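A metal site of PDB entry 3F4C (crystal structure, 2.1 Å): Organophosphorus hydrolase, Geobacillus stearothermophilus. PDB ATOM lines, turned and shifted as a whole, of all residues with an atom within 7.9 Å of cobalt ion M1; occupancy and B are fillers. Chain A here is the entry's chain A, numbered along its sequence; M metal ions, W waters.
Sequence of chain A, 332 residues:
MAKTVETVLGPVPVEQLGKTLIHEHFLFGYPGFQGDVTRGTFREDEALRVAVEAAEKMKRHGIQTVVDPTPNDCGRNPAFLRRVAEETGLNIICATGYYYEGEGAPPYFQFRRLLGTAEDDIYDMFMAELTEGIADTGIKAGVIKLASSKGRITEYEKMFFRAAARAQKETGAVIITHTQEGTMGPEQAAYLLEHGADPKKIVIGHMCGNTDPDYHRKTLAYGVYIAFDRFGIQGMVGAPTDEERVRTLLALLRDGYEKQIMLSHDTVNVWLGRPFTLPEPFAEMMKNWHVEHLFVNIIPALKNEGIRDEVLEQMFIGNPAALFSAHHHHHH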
ATOM      1  N   HIS A  23     -12.099  25.161  22.812  1.00  0.00           N
ATOM      2  CA  HIS A  23     -11.372  23.897  22.761  1.00  0.00           C
ATOM      3  C   HIS A  23      -9.915  24.058  22.408  1.00  0.00           C
ATOM      4  O   HIS A  23      -9.573  24.063  21.236  1.00  0.00           O
ATOM      5  CB  HIS A  23     -12.056  22.941  21.755  1.00  0.00           C
ATOM      6  CG  HIS A  23     -11.598  21.517  21.830  1.00  0.00           C
ATOM      7  ND1 HIS A  23     -12.470  20.444  21.757  1.00  0.00           N
ATOM      8  CD2 HIS A  23     -10.356  20.973  21.935  1.00  0.00           C
ATOM      9  CE1 HIS A  23     -11.792  19.315  21.815  1.00  0.00           C
ATOM     10  NE2 HIS A  23     -10.503  19.605  21.921  1.00  0.00           N
ATOM     11  N   HIS A  25      -5.729  22.971  23.952  1.00  0.00           N
ATOM     12  CA  HIS A  25      -4.956  22.197  24.911  1.00  0.00           C
ATOM     13  C   HIS A  25      -3.641  22.874  25.233  1.00  0.00           C
ATOM     14  O   HIS A  25      -2.825  23.092  24.349  1.00  0.00           O
ATOM     15  CB  HIS A  25      -4.604  20.814  24.362  1.00  0.00           C
ATOM     16  CG  HIS A  25      -5.796  19.987  23.999  1.00  0.00           C
ATOM     17  ND1 HIS A  25      -6.469  19.196  24.920  1.00  0.00           N
ATOM     18  CD2 HIS A  25      -6.452  19.837  22.837  1.00  0.00           C
ATOM     19  CE1 HIS A  25      -7.496  18.619  24.326  1.00  0.00           C
ATOM     20  NE2 HIS A  25      -7.499  18.995  23.062  1.00  0.00           N
ATOM     21  N   PHE A  28      -0.820  18.281  26.210  1.00  0.00           N
ATOM     22  CA  PHE A  28      -1.489  17.085  25.735  1.00  0.00           C
ATOM     23  C   PHE A  28      -0.578  15.910  25.370  1.00  0.00           C
ATOM     24  O   PHE A  28       0.474  16.083  24.758  1.00  0.00           O
ATOM     25  CB  PHE A  28      -2.372  17.411  24.533  1.00  0.00           C
ATOM     26  CG  PHE A  28      -3.115  16.220  24.002  1.00  0.00           C
ATOM     27  CD1 PHE A  28      -2.527  15.361  23.086  1.00  0.00           C
ATOM     28  CD2 PHE A  28      -4.421  15.934  24.451  1.00  0.00           C
ATOM     29  CE1 PHE A  28      -3.213  14.257  22.621  1.00  0.00           C
ATOM     30  CE2 PHE A  28      -5.096  14.861  23.992  1.00  0.00           C
ATOM     31  CZ  PHE A  28      -4.488  14.001  23.065  1.00  0.00           C
ATOM     32  N   TYR A  30      -0.893  11.676  23.973  1.00  0.00           N
ATOM     33  CA  TYR A  30      -1.678  10.510  23.562  1.00  0.00           C
ATOM     34  C   TYR A  30      -1.420   9.431  24.639  1.00  0.00           C
ATOM     35  O   TYR A  30      -0.278   9.249  25.062  1.00  0.00           O
ATOM     36  CB  TYR A  30      -1.185   9.995  22.199  1.00  0.00           C
ATOM     37  CG  TYR A  30      -1.740  10.779  21.034  1.00  0.00           C
ATOM     38  CD1 TYR A  30      -3.101  10.750  20.740  1.00  0.00           C
ATOM     39  CD2 TYR A  30      -0.918  11.571  20.244  1.00  0.00           C
ATOM     40  CE1 TYR A  30      -3.641  11.488  19.691  1.00  0.00           C
ATOM     41  CE2 TYR A  30      -1.428  12.316  19.182  1.00  0.00           C
ATOM     42  CZ  TYR A  30      -2.799  12.270  18.911  1.00  0.00           C
ATOM     43  OH  TYR A  30      -3.325  13.040  17.887  1.00  0.00           O
ATOM     44  N   PRO A  69     -10.147  20.916  27.335  1.00  0.00           N
ATOM     45  CA  PRO A  69     -10.762  19.640  27.653  1.00  0.00           C
ATOM     46  C   PRO A  69      -9.870  18.408  27.658  1.00  0.00           C
ATOM     47  O   PRO A  69     -10.332  17.296  27.432  1.00  0.00           O
ATOM     48  CB  PRO A  69     -11.888  19.560  26.634  1.00  0.00           C
ATOM     49  CG  PRO A  69     -11.231  20.152  25.384  1.00  0.00           C
ATOM     50  CD  PRO A  69     -10.234  21.201  25.885  1.00  0.00           C
ATOM     51  N   PRO A  71      -8.481  15.127  28.251  1.00  0.00           N
ATOM     52  CA  PRO A  71      -9.024  13.993  29.022  1.00  0.00           C
ATOM     53  C   PRO A  71      -8.073  13.522  30.116  1.00  0.00           C
ATOM     54  O   PRO A  71      -6.859  13.731  30.025  1.00  0.00           O
ATOM     55  CB  PRO A  71      -9.265  12.917  27.952  1.00  0.00           C
ATOM     56  CG  PRO A  71      -9.533  13.761  26.671  1.00  0.00           C
ATOM     57  CD  PRO A  71      -8.428  14.805  26.803  1.00  0.00           C
ATOM     58  N   TYR A  99     -10.366   9.656  26.946  1.00  0.00           N
ATOM     59  CA  TYR A  99     -10.400   9.737  25.486  1.00  0.00           C
ATOM     60  C   TYR A  99     -11.192   8.598  24.781  1.00  0.00           C
ATOM     61  O   TYR A  99     -11.500   7.561  25.404  1.00  0.00           O
ATOM     62  CB  TYR A  99      -9.007   9.846  24.921  1.00  0.00           C
ATOM     63  CG  TYR A  99      -9.029  10.751  23.709  1.00  0.00           C
ATOM     64  CD1 TYR A  99     -10.116  11.610  23.487  1.00  0.00           C
ATOM     65  CD2 TYR A  99      -7.982  10.745  22.775  1.00  0.00           C
ATOM     66  CE1 TYR A  99     -10.185  12.418  22.369  1.00  0.00           C
ATOM     67  CE2 TYR A  99      -8.042  11.552  21.657  1.00  0.00           C
ATOM     68  CZ  TYR A  99      -9.149  12.383  21.450  1.00  0.00           C
ATOM     69  OH  TYR A  99      -9.230  13.170  20.325  1.00  0.00           O
ATOM     70  N   TYR A 100     -11.553   8.779  23.502  1.00  0.00           N
ATOM     71  CA  TYR A 100     -12.330   7.761  22.801  1.00  0.00           C
ATOM     72  C   TYR A 100     -11.538   6.449  22.701  1.00  0.00           C
ATOM     73  O   TYR A 100     -10.317   6.453  22.835  1.00  0.00           O
ATOM     74  CB  TYR A 100     -12.806   8.266  21.421  1.00  0.00           C
ATOM     75  CG  TYR A 100     -11.837   8.136  20.266  1.00  0.00           C
ATOM     76  CD1 TYR A 100     -10.816   9.052  20.065  1.00  0.00           C
ATOM     77  CD2 TYR A 100     -11.967   7.086  19.356  1.00  0.00           C
ATOM     78  CE1 TYR A 100      -9.943   8.921  18.975  1.00  0.00           C
ATOM     79  CE2 TYR A 100     -11.103   6.946  18.279  1.00  0.00           C
ATOM     80  CZ  TYR A 100     -10.091   7.865  18.098  1.00  0.00           C
ATOM     81  OH  TYR A 100      -9.239   7.687  17.026  1.00  0.00           O
ATOM     82  N   KCX A 145     -15.970  15.704  29.588  1.00  0.00           N
ATOM     83  CA  KCX A 145     -15.476  15.482  28.241  1.00  0.00           C
ATOM     84  CB  KCX A 145     -13.966  15.723  28.228  1.00  0.00           C
ATOM     85  CG  KCX A 145     -13.295  15.358  26.896  1.00  0.00           C
ATOM     86  CD  KCX A 145     -13.815  16.226  25.770  1.00  0.00           C
ATOM     87  CE  KCX A 145     -12.596  16.633  24.960  1.00  0.00           C
ATOM     88  NZ  KCX A 145     -12.545  15.967  23.672  1.00  0.00           N
ATOM     89  C   KCX A 145     -15.786  14.059  27.719  1.00  0.00           C
ATOM     90  O   KCX A 145     -15.401  13.074  28.333  1.00  0.00           O
ATOM     91  CX  KCX A 145     -11.561  16.108  22.776  1.00  0.00           C
ATOM     92  OQ1 KCX A 145     -11.657  15.518  21.680  1.00  0.00           O
ATOM     93  OQ2 KCX A 145     -10.423  16.609  23.100  1.00  0.00           O
ATOM     94  N   LEU A 146     -16.478  13.964  26.574  1.00  0.00           N
ATOM     95  CA  LEU A 146     -16.827  12.675  25.988  1.00  0.00           C
ATOM     96  C   LEU A 146     -16.315  12.554  24.558  1.00  0.00           C
ATOM     97  O   LEU A 146     -16.131  13.568  23.884  1.00  0.00           O
ATOM     98  CB  LEU A 146     -18.359  12.499  25.945  1.00  0.00           C
ATOM     99  CG  LEU A 146     -19.112  12.522  27.261  1.00  0.00           C
ATOM    100  CD1 LEU A 146     -20.622  12.566  26.948  1.00  0.00           C
ATOM    101  CD2 LEU A 146     -18.753  11.271  28.099  1.00  0.00           C
ATOM    102  N   ALA A 147     -16.133  11.327  24.093  1.00  0.00           N
ATOM    103  CA  ALA A 147     -15.693  11.063  22.714  1.00  0.00           C
ATOM    104  C   ALA A 147     -16.282   9.734  22.158  1.00  0.00           C
ATOM    105  O   ALA A 147     -16.539   8.801  22.908  1.00  0.00           O
ATOM    106  CB  ALA A 147     -14.134  11.005  22.662  1.00  0.00           C
ATOM    107  N   THR A 177     -18.201  17.140  23.643  1.00  0.00           N
ATOM    108  CA  THR A 177     -17.836  15.856  23.082  1.00  0.00           C
ATOM    109  C   THR A 177     -16.918  16.036  21.904  1.00  0.00           C
ATOM    110  O   THR A 177     -16.729  17.153  21.420  1.00  0.00           O
ATOM    111  CB  THR A 177     -19.038  15.107  22.519  1.00  0.00           C
ATOM    112  OG1 THR A 177     -19.290  15.604  21.207  1.00  0.00           O
ATOM    113  CG2 THR A 177     -20.272  15.312  23.391  1.00  0.00           C
ATOM    114  N   HIS A 178     -16.392  14.911  21.446  1.00  0.00           N
ATOM    115  CA  HIS A 178     -15.541  14.852  20.279  1.00  0.00           C
ATOM    116  C   HIS A 178     -16.132  13.756  19.384  1.00  0.00           C
ATOM    117  O   HIS A 178     -16.568  12.727  19.874  1.00  0.00           O
ATOM    118  CB  HIS A 178     -14.072  14.551  20.705  1.00  0.00           C
ATOM    119  CG  HIS A 178     -13.394  13.483  19.908  1.00  0.00           C
ATOM    120  ND1 HIS A 178     -12.058  13.559  19.572  1.00  0.00           N
ATOM    121  CD2 HIS A 178     -13.823  12.281  19.438  1.00  0.00           C
ATOM    122  CE1 HIS A 178     -11.692  12.457  18.930  1.00  0.00           C
ATOM    123  NE2 HIS A 178     -12.747  11.667  18.826  1.00  0.00           N
ATOM    124  N   THR A 179     -16.190  14.009  18.098  1.00  0.00           N
ATOM    125  CA  THR A 179     -16.661  12.996  17.165  1.00  0.00           C
ATOM    126  C   THR A 179     -15.407  12.676  16.356  1.00  0.00           C
ATOM    127  O   THR A 179     -14.527  13.529  16.182  1.00  0.00           O
ATOM    128  CB  THR A 179     -17.801  13.522  16.239  1.00  0.00           C
ATOM    129  OG1 THR A 179     -17.409  14.723  15.581  1.00  0.00           O
ATOM    130  CG2 THR A 179     -19.067  13.781  17.046  1.00  0.00           C
ATOM    131  N   GLN A 180     -15.337  11.439  15.869  1.00  0.00           N
ATOM    132  CA  GLN A 180     -14.183  10.988  15.122  1.00  0.00           C
ATOM    133  C   GLN A 180     -14.463  11.002  13.625  1.00  0.00           C
ATOM    134  O   GLN A 180     -15.397  10.343  13.125  1.00  0.00           O
ATOM    135  CB  GLN A 180     -13.802   9.582  15.583  1.00  0.00           C
ATOM    136  CG  GLN A 180     -12.499   9.051  15.037  1.00  0.00           C
ATOM    137  CD  GLN A 180     -11.314   9.921  15.426  1.00  0.00           C
ATOM    138  OE1 GLN A 180     -11.360  10.664  16.423  1.00  0.00           O
ATOM    139  NE2 GLN A 180     -10.241   9.841  14.641  1.00  0.00           N
ATOM    140  N   GLY A 205     -18.513  18.345  19.418  1.00  0.00           N
ATOM    141  CA  GLY A 205     -17.301  18.853  18.788  1.00  0.00           C
ATOM    142  C   GLY A 205     -16.869  18.187  17.496  1.00  0.00           C
ATOM    143  O   GLY A 205     -17.427  17.177  17.094  1.00  0.00           O
ATOM    144  N   HIS A 206     -15.814  18.751  16.880  1.00  0.00           N
ATOM    145  CA  HIS A 206     -15.264  18.304  15.596  1.00  0.00           C
ATOM    146  C   HIS A 206     -16.315  18.184  14.506  1.00  0.00           C
ATOM    147  O   HIS A 206     -16.155  17.389  13.600  1.00  0.00           O
ATOM    148  CB  HIS A 206     -14.571  16.958  15.697  1.00  0.00           C
ATOM    149  CG  HIS A 206     -13.433  16.939  16.646  1.00  0.00           C
ATOM    150  ND1 HIS A 206     -13.042  18.060  17.359  1.00  0.00           N
ATOM    151  CD2 HIS A 206     -12.630  15.928  17.055  1.00  0.00           C
ATOM    152  CE1 HIS A 206     -12.052  17.736  18.171  1.00  0.00           C
ATOM    153  NE2 HIS A 206     -11.784  16.451  18.010  1.00  0.00           N
ATOM    154  N   ASP A 229     -14.095  23.138  15.679  1.00  0.00           N
ATOM    155  CA  ASP A 229     -12.991  23.385  16.579  1.00  0.00           C
ATOM    156  C   ASP A 229     -11.619  22.878  16.167  1.00  0.00           C
ATOM    157  O   ASP A 229     -10.764  22.671  17.004  1.00  0.00           O
ATOM    158  CB  ASP A 229     -13.367  22.824  17.979  1.00  0.00           C
ATOM    159  CG  ASP A 229     -13.821  21.367  17.904  1.00  0.00           C
ATOM    160  OD1 ASP A 229     -13.421  20.688  16.928  1.00  0.00           O
ATOM    161  OD2 ASP A 229     -14.575  20.889  18.814  1.00  0.00           O
ATOM    162  N   ARG A 230     -11.402  22.690  14.874  1.00  0.00           N
ATOM    163  CA  ARG A 230     -10.121  22.203  14.445  1.00  0.00           C
ATOM    164  C   ARG A 230      -9.557  23.064  13.321  1.00  0.00           C
ATOM    165  O   ARG A 230      -8.823  22.571  12.464  1.00  0.00           O
ATOM    166  CB  ARG A 230     -10.254  20.729  14.039  1.00  0.00           C
ATOM    167  CG  ARG A 230     -10.414  19.787  15.247  1.00  0.00           C
ATOM    168  CD  ARG A 230     -10.825  18.383  14.861  1.00  0.00           C
ATOM    169  NE  ARG A 230      -9.779  17.629  14.165  1.00  0.00           N
ATOM    170  CZ  ARG A 230      -8.721  17.064  14.739  1.00  0.00           C
ATOM    171  NH1 ARG A 230      -8.539  17.172  16.046  1.00  0.00           N
ATOM    172  NH2 ARG A 230      -7.836  16.389  13.994  1.00  0.00           N
ATOM    173  N   ASP A 266      -8.344  23.626  18.556  1.00  0.00           N
ATOM    174  CA  ASP A 266      -7.913  22.340  19.111  1.00  0.00           C
ATOM    175  C   ASP A 266      -6.385  22.189  19.112  1.00  0.00           C
ATOM    176  O   ASP A 266      -5.855  21.115  18.839  1.00  0.00           O
ATOM    177  CB  ASP A 266      -8.570  21.197  18.326  1.00  0.00           C
ATOM    178  CG  ASP A 266      -8.404  19.853  19.006  1.00  0.00           C
ATOM    179  OD1 ASP A 266      -7.935  19.814  20.160  1.00  0.00           O
ATOM    180  OD2 ASP A 266      -8.737  18.819  18.360  1.00  0.00           O
HETATM  181 CO    CO M   1     -10.504  15.456  19.859  1.00  0.00          CO
HETATM  182 CO    CO M   2      -8.860  18.176  21.700  1.00  0.00          CO
HETATM  183  O   HOH W   1      -9.485  17.066  20.082  1.00  0.00           O
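OQ2 of KCX 145 sits close to a ring nitrogen (NE2) of His 23, at 3.2 Å. OD1 of Asp 229 is in hydrogen-bond range of ND1 of His 206 (2.7 Å). ND1 of His 178 lies close to OH of Tyr 99. A ring nitrogen (NE2) of His 178 lies within hydrogen-bond range of the side-chain amide oxygen of Gln 180 (3.0 Å). The backbone NH (N) of His 178 is in hydrogen-bond range of the backbone carbonyl oxygen (O) of Leu 146 (2.8 Å).
Within 4 Å of cobalt ion M1: Tyr 99, KCX 145, His 178 and His 206. The nearest printed residue that does not touch cobalt ion M1 is Asp 266 (4.1 Å).
Cobalt ion M1 is bound by water W1 (1.9 Å), OQ1 of KCX 145 (2.2 Å), a ring nitrogen (NE2) of His 206 (2.5 Å) and a ring nitrogen (ND1) of His 178 (2.5 Å). Slightly farther from cobalt ion M1 lies OH of Tyr 99 (2.7 Å).
Water W1 lies within hydrogen-bond range of OD2 of Asp 266 and OQ2 of KCX 145.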
